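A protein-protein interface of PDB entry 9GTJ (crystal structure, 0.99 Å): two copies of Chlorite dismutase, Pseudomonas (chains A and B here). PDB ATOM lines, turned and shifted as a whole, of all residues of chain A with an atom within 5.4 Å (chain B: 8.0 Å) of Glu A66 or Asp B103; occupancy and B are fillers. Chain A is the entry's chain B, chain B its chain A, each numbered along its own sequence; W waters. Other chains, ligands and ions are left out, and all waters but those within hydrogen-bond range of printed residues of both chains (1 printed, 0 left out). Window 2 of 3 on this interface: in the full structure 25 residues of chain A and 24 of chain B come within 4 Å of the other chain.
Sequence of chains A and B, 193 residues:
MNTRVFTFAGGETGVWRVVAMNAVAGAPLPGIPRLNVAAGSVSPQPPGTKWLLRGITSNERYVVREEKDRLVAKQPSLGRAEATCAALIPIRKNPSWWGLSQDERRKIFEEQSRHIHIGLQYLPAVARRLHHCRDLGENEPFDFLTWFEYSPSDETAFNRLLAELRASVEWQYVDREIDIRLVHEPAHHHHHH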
ATOM      1  N   VAL A  63     -27.462 -24.576  21.264  1.00  0.00           N
ATOM      2  CA  VAL A  63     -27.086 -25.631  22.199  1.00  0.00           C
ATOM      3  C   VAL A  63     -25.588 -25.820  22.251  1.00  0.00           C
ATOM      4  O   VAL A  63     -24.942 -25.975  21.209  1.00  0.00           O
ATOM      5  CB  VAL A  63     -27.682 -26.989  21.713  1.00  0.00           C
ATOM      6  CG1 VAL A  63     -27.058 -28.246  22.341  1.00  0.00           C
ATOM      7  CG2 VAL A  63     -29.153 -27.029  21.875  1.00  0.00           C
ATOM      8  N   VAL A  64     -25.059 -25.891  23.469  1.00  0.00           N
ATOM      9  CA  VAL A  64     -23.660 -26.229  23.651  1.00  0.00           C
ATOM     10  C   VAL A  64     -23.543 -27.714  23.995  1.00  0.00           C
ATOM     11  O   VAL A  64     -24.514 -28.352  24.394  1.00  0.00           O
ATOM     12  CB  VAL A  64     -22.981 -25.329  24.689  1.00  0.00           C
ATOM     13  CG1 VAL A  64     -23.195 -23.871  24.321  1.00  0.00           C
ATOM     14  CG2 VAL A  64     -23.440 -25.625  26.095  1.00  0.00           C
ATOM     15  N   ARG A  65     -22.334 -28.283  23.833  1.00  0.00           N
ATOM     16  CA  ARG A  65     -22.171 -29.730  23.987  1.00  0.00           C
ATOM     17  C   ARG A  65     -22.721 -30.223  25.330  1.00  0.00           C
ATOM     18  O   ARG A  65     -23.374 -31.268  25.395  1.00  0.00           O
ATOM     19  CB  ARG A  65     -20.709 -30.136  23.772  1.00  0.00           C
ATOM     20  CG  ARG A  65     -20.479 -31.649  23.930  1.00  0.00           C
ATOM     21  CD  ARG A  65     -21.227 -32.526  22.908  1.00  0.00           C
ATOM     22  NE  ARG A  65     -20.846 -32.339  21.492  1.00  0.00           N
ATOM     23  CZ  ARG A  65     -21.359 -32.974  20.422  1.00  0.00           C
ATOM     24  NH1 ARG A  65     -22.319 -33.876  20.563  1.00  0.00           N
ATOM     25  NH2 ARG A  65     -20.864 -32.718  19.212  1.00  0.00           N
ATOM     26  N   GLU A  66     -22.450 -29.505  26.429  1.00  0.00           N
ATOM     27  CA  GLU A  66     -22.890 -29.965  27.736  1.00  0.00           C
ATOM     28  C   GLU A  66     -24.424 -30.046  27.802  1.00  0.00           C
ATOM     29  O   GLU A  66     -24.985 -30.938  28.447  1.00  0.00           O
ATOM     30  CB  GLU A  66     -22.312 -29.009  28.785  1.00  0.00           C
ATOM     31  CG  GLU A  66     -20.879 -28.501  28.500  1.00  0.00           C
ATOM     32  CD  GLU A  66     -20.610 -27.240  27.652  1.00  0.00           C
ATOM     33  OE1 GLU A  66     -20.558 -26.065  28.276  1.00  0.00           O
ATOM     34  OE2 GLU A  66     -20.334 -27.393  26.374  1.00  0.00           O
ATOM     35  N   GLU A  67     -25.095 -29.072  27.171  1.00  0.00           N
ATOM     36  CA  GLU A  67     -26.557 -29.085  27.104  1.00  0.00           C
ATOM     37  C   GLU A  67     -27.044 -30.244  26.246  1.00  0.00           C
ATOM     38  O   GLU A  67     -28.012 -30.916  26.593  1.00  0.00           O
ATOM     39  CB  GLU A  67     -27.057 -27.755  26.553  1.00  0.00           C
ATOM     40  CG  GLU A  67     -26.878 -26.611  27.534  1.00  0.00           C
ATOM     41  CD  GLU A  67     -27.003 -25.222  26.929  1.00  0.00           C
ATOM     42  OE1 GLU A  67     -26.848 -25.036  25.697  1.00  0.00           O
ATOM     43  OE2 GLU A  67     -27.169 -24.273  27.746  1.00  0.00           O
ATOM     44  N   LYS A  68     -26.382 -30.445  25.106  1.00  0.00           N
ATOM     45  CA  LYS A  68     -26.742 -31.551  24.230  1.00  0.00           C
ATOM     46  C   LYS A  68     -26.701 -32.871  24.991  1.00  0.00           C
ATOM     47  O   LYS A  68     -27.580 -33.719  24.860  1.00  0.00           O
ATOM     48  CB  LYS A  68     -25.798 -31.589  23.030  1.00  0.00           C
ATOM     49  CG  LYS A  68     -26.142 -32.647  21.999  1.00  0.00           C
ATOM     50  CD  LYS A  68     -27.582 -32.612  21.569  1.00  0.00           C
ATOM     51  CE  LYS A  68     -27.876 -33.505  20.384  1.00  0.00           C
ATOM     52  NZ  LYS A  68     -27.014 -33.195  19.221  1.00  0.00           N
ATOM     53  N   ASP A  69     -25.632 -33.056  25.767  1.00  0.00           N
ATOM     54  CA  ASP A  69     -25.513 -34.313  26.494  1.00  0.00           C
ATOM     55  C   ASP A  69     -26.655 -34.509  27.493  1.00  0.00           C
ATOM     56  O   ASP A  69     -27.170 -35.628  27.647  1.00  0.00           O
ATOM     57  CB  ASP A  69     -24.117 -34.401  27.089  1.00  0.00           C
ATOM     58  CG  ASP A  69     -23.063 -34.799  26.062  1.00  0.00           C
ATOM     59  OD1 ASP A  69     -23.373 -35.687  25.184  1.00  0.00           O
ATOM     60  OD2 ASP A  69     -21.928 -34.428  26.235  1.00  0.00           O
ATOM     61  N   ARG A  70     -27.094 -33.434  28.156  1.00  0.00           N
ATOM     62  CA  ARG A  70     -28.234 -33.524  29.057  1.00  0.00           C
ATOM     63  C   ARG A  70     -29.515 -33.886  28.301  1.00  0.00           C
ATOM     64  O   ARG A  70     -30.298 -34.708  28.776  1.00  0.00           O
ATOM     65  CB  ARG A  70     -28.441 -32.213  29.824  1.00  0.00           C
ATOM     66  CG  ARG A  70     -27.423 -31.966  30.925  1.00  0.00           C
ATOM     67  CD  ARG A  70     -27.170 -30.542  31.458  1.00  0.00           C
ATOM     68  NE  ARG A  70     -28.131 -29.475  31.193  1.00  0.00           N
ATOM     69  CZ  ARG A  70     -27.825 -28.186  30.971  1.00  0.00           C
ATOM     70  NH1 ARG A  70     -26.562 -27.787  31.051  1.00  0.00           N
ATOM     71  NH2 ARG A  70     -28.779 -27.294  30.691  1.00  0.00           N
ATOM     72  N   TYR B  62     -22.648 -16.831  14.182  1.00  0.00           N
ATOM     73  CA  TYR B  62     -21.432 -16.880  14.993  1.00  0.00           C
ATOM     74  C   TYR B  62     -21.001 -15.512  15.519  1.00  0.00           C
ATOM     75  O   TYR B  62     -20.487 -15.427  16.635  1.00  0.00           O
ATOM     76  CB  TYR B  62     -20.239 -17.481  14.216  1.00  0.00           C
ATOM     77  CG  TYR B  62     -20.486 -18.924  13.825  1.00  0.00           C
ATOM     78  CD1 TYR B  62     -20.567 -19.919  14.783  1.00  0.00           C
ATOM     79  CD2 TYR B  62     -20.712 -19.280  12.503  1.00  0.00           C
ATOM     80  CE1 TYR B  62     -20.902 -21.217  14.432  1.00  0.00           C
ATOM     81  CE2 TYR B  62     -21.035 -20.570  12.138  1.00  0.00           C
ATOM     82  CZ  TYR B  62     -21.142 -21.551  13.106  1.00  0.00           C
ATOM     83  OH  TYR B  62     -21.486 -22.833  12.810  1.00  0.00           O
ATOM     84  N   LEU B 100     -21.762 -31.082  14.881  1.00  0.00           N
ATOM     85  CA  LEU B 100     -21.147 -30.457  16.045  1.00  0.00           C
ATOM     86  C   LEU B 100     -22.134 -29.494  16.706  1.00  0.00           C
ATOM     87  O   LEU B 100     -23.002 -28.925  16.046  1.00  0.00           O
ATOM     88  CB  LEU B 100     -19.884 -29.688  15.655  1.00  0.00           C
ATOM     89  CG  LEU B 100     -18.734 -30.515  15.069  1.00  0.00           C
ATOM     90  CD1 LEU B 100     -17.605 -29.590  14.660  1.00  0.00           C
ATOM     91  CD2 LEU B 100     -18.239 -31.567  16.040  1.00  0.00           C
ATOM     92  N   SER B 101     -21.935 -29.275  18.013  1.00  0.00           N
ATOM     93  CA  SER B 101     -22.747 -28.322  18.750  1.00  0.00           C
ATOM     94  C   SER B 101     -22.263 -26.896  18.488  1.00  0.00           C
ATOM     95  O   SER B 101     -21.239 -26.661  17.839  1.00  0.00           O
ATOM     96  CB  SER B 101     -22.757 -28.672  20.225  1.00  0.00           C
ATOM     97  OG  SER B 101     -23.476 -29.881  20.433  1.00  0.00           O
ATOM     98  N   GLN B 102     -23.038 -25.925  18.975  1.00  0.00           N
ATOM     99  CA  GLN B 102     -22.771 -24.542  18.605  1.00  0.00           C
ATOM    100  C   GLN B 102     -21.442 -24.043  19.149  1.00  0.00           C
ATOM    101  O   GLN B 102     -20.724 -23.322  18.465  1.00  0.00           O
ATOM    102  CB  GLN B 102     -23.913 -23.674  19.088  1.00  0.00           C
ATOM    103  CG  GLN B 102     -23.738 -22.185  18.833  1.00  0.00           C
ATOM    104  CD  GLN B 102     -23.653 -21.818  17.376  1.00  0.00           C
ATOM    105  OE1 GLN B 102     -24.162 -22.534  16.504  1.00  0.00           O
ATOM    106  NE2 GLN B 102     -23.055 -20.664  17.115  1.00  0.00           N
ATOM    107  N   ASP B 103     -21.128 -24.380  20.398  1.00  0.00           N
ATOM    108  CA  ASP B 103     -19.870 -23.962  20.972  1.00  0.00           C
ATOM    109  C   ASP B 103     -18.686 -24.556  20.217  1.00  0.00           C
ATOM    110  O   ASP B 103     -17.655 -23.893  20.038  1.00  0.00           O
ATOM    111  CB  ASP B 103     -19.774 -24.301  22.466  1.00  0.00           C
ATOM    112  CG  ASP B 103     -19.992 -25.745  22.869  1.00  0.00           C
ATOM    113  OD1 ASP B 103     -20.690 -26.475  22.140  1.00  0.00           O
ATOM    114  OD2 ASP B 103     -19.469 -26.119  23.945  1.00  0.00           O
ATOM    115  N   GLU B 104     -18.794 -25.809  19.804  1.00  0.00           N
ATOM    116  CA  GLU B 104     -17.723 -26.467  19.084  1.00  0.00           C
ATOM    117  C   GLU B 104     -17.452 -25.760  17.767  1.00  0.00           C
ATOM    118  O   GLU B 104     -16.303 -25.548  17.376  1.00  0.00           O
ATOM    119  CB  GLU B 104     -18.075 -27.933  18.872  1.00  0.00           C
ATOM    120  CG  GLU B 104     -18.097 -28.725  20.157  1.00  0.00           C
ATOM    121  CD  GLU B 104     -18.724 -30.111  20.062  1.00  0.00           C
ATOM    122  OE1 GLU B 104     -19.456 -30.393  19.106  1.00  0.00           O
ATOM    123  OE2 GLU B 104     -18.503 -30.914  20.993  1.00  0.00           O
ATOM    124  N   ARG B 105     -18.510 -25.413  17.023  1.00  0.00           N
ATOM    125  CA  ARG B 105     -18.345 -24.728  15.751  1.00  0.00           C
ATOM    126  C   ARG B 105     -17.839 -23.308  15.933  1.00  0.00           C
ATOM    127  O   ARG B 105     -16.974 -22.879  15.164  1.00  0.00           O
ATOM    128  CB  ARG B 105     -19.644 -24.771  14.951  1.00  0.00           C
ATOM    129  CG  ARG B 105     -19.848 -26.125  14.291  1.00  0.00           C
ATOM    130  CD  ARG B 105     -21.125 -26.256  13.478  1.00  0.00           C
ATOM    131  NE  ARG B 105     -22.298 -26.618  14.273  1.00  0.00           N
ATOM    132  CZ  ARG B 105     -23.167 -25.783  14.837  1.00  0.00           C
ATOM    133  NH1 ARG B 105     -23.183 -24.486  14.556  1.00  0.00           N
ATOM    134  NH2 ARG B 105     -24.038 -26.272  15.690  1.00  0.00           N
ATOM    135  N   ARG B 106     -18.345 -22.572  16.922  1.00  0.00           N
ATOM    136  CA  ARG B 106     -17.820 -21.217  17.142  1.00  0.00           C
ATOM    137  C   ARG B 106     -16.321 -21.258  17.466  1.00  0.00           C
ATOM    138  O   ARG B 106     -15.555 -20.423  17.002  1.00  0.00           O
ATOM    139  CB  ARG B 106     -18.594 -20.526  18.268  1.00  0.00           C
ATOM    140  CG  ARG B 106     -17.969 -19.242  18.807  1.00  0.00           C
ATOM    141  CD  ARG B 106     -17.811 -18.107  17.808  1.00  0.00           C
ATOM    142  NE  ARG B 106     -16.936 -17.080  18.372  1.00  0.00           N
ATOM    143  CZ  ARG B 106     -16.796 -15.822  17.949  1.00  0.00           C
ATOM    144  NH1 ARG B 106     -17.624 -15.287  17.076  1.00  0.00           N
ATOM    145  NH2 ARG B 106     -15.803 -15.079  18.420  1.00  0.00           N
ATOM    146  N   LYS B 107     -15.921 -22.236  18.289  1.00  0.00           N
ATOM    147  CA  LYS B 107     -14.506 -22.349  18.634  1.00  0.00           C
ATOM    148  C   LYS B 107     -13.656 -22.552  17.381  1.00  0.00           C
ATOM    149  O   LYS B 107     -12.618 -21.919  17.218  1.00  0.00           O
ATOM    150  CB  LYS B 107     -14.292 -23.477  19.638  1.00  0.00           C
ATOM    151  CG  LYS B 107     -12.819 -23.708  19.957  1.00  0.00           C
ATOM    152  CD  LYS B 107     -12.591 -24.709  21.027  1.00  0.00           C
ATOM    153  CE  LYS B 107     -11.116 -24.842  21.321  1.00  0.00           C
ATOM    154  NZ  LYS B 107     -10.893 -25.734  22.478  1.00  0.00           N
ATOM    155  N   ILE B 108     -14.070 -23.463  16.499  1.00  0.00           N
ATOM    156  CA  ILE B 108     -13.325 -23.696  15.274  1.00  0.00           C
ATOM    157  C   ILE B 108     -13.304 -22.450  14.403  1.00  0.00           C
ATOM    158  O   ILE B 108     -12.262 -22.068  13.876  1.00  0.00           O
ATOM    159  CB  ILE B 108     -13.868 -24.917  14.519  1.00  0.00           C
ATOM    160  CG1 ILE B 108     -13.599 -26.210  15.305  1.00  0.00           C
ATOM    161  CG2 ILE B 108     -13.316 -24.978  13.103  1.00  0.00           C
ATOM    162  CD1 ILE B 108     -14.522 -27.358  14.933  1.00  0.00           C
ATOM    163  N   PHE B 109     -14.477 -21.847  14.206  1.00  0.00           N
ATOM    164  CA  PHE B 109     -14.652 -20.764  13.259  1.00  0.00           C
ATOM    165  C   PHE B 109     -13.825 -19.539  13.641  1.00  0.00           C
ATOM    166  O   PHE B 109     -13.134 -18.991  12.767  1.00  0.00           O
ATOM    167  CB  PHE B 109     -16.147 -20.427  13.209  1.00  0.00           C
ATOM    168  CG  PHE B 109     -16.457 -19.244  12.337  1.00  0.00           C
ATOM    169  CD1 PHE B 109     -16.509 -19.369  10.958  1.00  0.00           C
ATOM    170  CD2 PHE B 109     -16.717 -18.014  12.895  1.00  0.00           C
ATOM    171  CE1 PHE B 109     -16.785 -18.272  10.165  1.00  0.00           C
ATOM    172  CE2 PHE B 109     -16.955 -16.911  12.102  1.00  0.00           C
ATOM    173  CZ  PHE B 109     -16.985 -17.056  10.747  1.00  0.00           C
ATOM    174  N   GLU B 110     -13.892 -19.131  14.910  1.00  0.00           N
ATOM    175  CA  GLU B 110     -13.228 -17.882  15.255  1.00  0.00           C
ATOM    176  C   GLU B 110     -12.057 -18.100  16.213  1.00  0.00           C
ATOM    177  O   GLU B 110     -10.962 -17.623  15.950  1.00  0.00           O
ATOM    178  CB  GLU B 110     -14.174 -16.820  15.815  1.00  0.00           C
ATOM    179  CG  GLU B 110     -13.486 -15.471  15.920  1.00  0.00           C
ATOM    180  CD  GLU B 110     -13.032 -14.926  14.576  1.00  0.00           C
ATOM    181  OE1 GLU B 110     -13.606 -15.343  13.555  1.00  0.00           O
ATOM    182  OE2 GLU B 110     -12.079 -14.072  14.536  1.00  0.00           O
ATOM    183  N   GLU B 111     -12.247 -18.761  17.356  1.00  0.00           N
ATOM    184  CA  GLU B 111     -11.160 -18.825  18.326  1.00  0.00           C
ATOM    185  C   GLU B 111      -9.934 -19.509  17.732  1.00  0.00           C
ATOM    186  O   GLU B 111      -8.817 -19.077  18.005  1.00  0.00           O
ATOM    187  CB  GLU B 111     -11.677 -19.411  19.638  1.00  0.00           C
ATOM    188  CG  GLU B 111     -12.315 -18.298  20.490  1.00  0.00           C
ATOM    189  CD  GLU B 111     -13.530 -17.598  19.868  1.00  0.00           C
ATOM    190  OE1 GLU B 111     -14.529 -18.292  19.572  1.00  0.00           O
ATOM    191  OE2 GLU B 111     -13.466 -16.342  19.622  1.00  0.00           O
ATOM    192  N   GLN B 112     -10.120 -20.594  16.978  1.00  0.00           N
ATOM    193  CA  GLN B 112      -9.027 -21.277  16.325  1.00  0.00           C
ATOM    194  C   GLN B 112      -8.703 -20.661  14.974  1.00  0.00           C
ATOM    195  O   GLN B 112      -7.564 -20.281  14.716  1.00  0.00           O
ATOM    196  CB  GLN B 112      -9.337 -22.764  16.206  1.00  0.00           C
ATOM    197  CG  GLN B 112      -9.429 -23.432  17.567  1.00  0.00           C
ATOM    198  CD  GLN B 112      -9.732 -24.910  17.530  1.00  0.00           C
ATOM    199  OE1 GLN B 112     -10.661 -25.388  16.926  1.00  0.00           O
ATOM    200  NE2 GLN B 112      -8.962 -25.682  18.261  1.00  0.00           N
HETATM  201  O   HOH W   1     -24.395 -31.761  18.647  1.00  0.00           O
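Ser B101 touches Val A63.
Val A64 touches Ser B101 (C to CB, 3.97 Å).
Val A64 touches Asp B103.
Leu B100 touches Arg A65.
Arg A65 touches Ser B101.
Lys A68 touches Ser B101 (CB to OG, 3.9 Å).
The side-chain carboxylate (OD2) of Asp B103 lies close to the side-chain carboxylate (OE2) of Glu A66 (2.9 Å).
The side-chain carboxylate (OE1) of Glu B104 is in salt-bridge range of the guanidinium group (NH2) of Arg A65, 2.7 Å away.
The side-chain carboxylate (OD1) of Asp B103 is in hydrogen-bond range of the backbone NH (N) of Arg A65, at 3.0 Å.
N of Gln B102 lies within hydrogen-bond range of O of Val A63.
Printed residues of chain B that touch a printed residue of chain A: Leu B100, Ser B101, Gln B102, Asp B103 and Glu B104.
Printed residues of chain A that touch a printed residue of chain B: Val A63, Val A64, Arg A65, Glu A66 and Lys A68.
Among the printed residues, 10 pairs touch across the chains.
Of chain B, only Asp B103 (2.9 Å) comes within 4 Å of Glu A66.
Asp B103 touches three residues of chain A.
Printed residues of chain B within 4 Å of Lys A68: Ser B101 (3.9 Å).
Of the printed residues of chain A, Leu B100 touches Arg A65.
Of the printed residues of chain B, Val A63 touches Ser B101 and Gln B102.
Of the printed residues of chain A, Gln B102 touches Val A63.
Of the printed residues of chain A, Ser B101 touches Val A63, Val A64, Arg A65 and Lys A68.
The nearest printed residue of chain B that does not touch Arg A65 is Gln B102 (5.4 Å).
Water W1 bridges the side-chain hydroxyl (OG) of Ser B101 and the side-chain amino group (NZ) of Lys A68.
OE1 of Gln B102 lies within hydrogen-bond range of NH1 of Arg B105 (2.9 Å).
The backbone NH (N) of Val A64 lies within hydrogen-bond range of the side-chain carboxylate (OE1) of Glu A67.
NH2 of Arg B105 sits at hydrogen-bond distance from O of Leu B100 (2.9 Å).
The backbone NH of Ser B101 lies within hydrogen-bond range of the side-chain carboxylate of Glu B104 (2.9 Å).
No position is printed for both chains.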
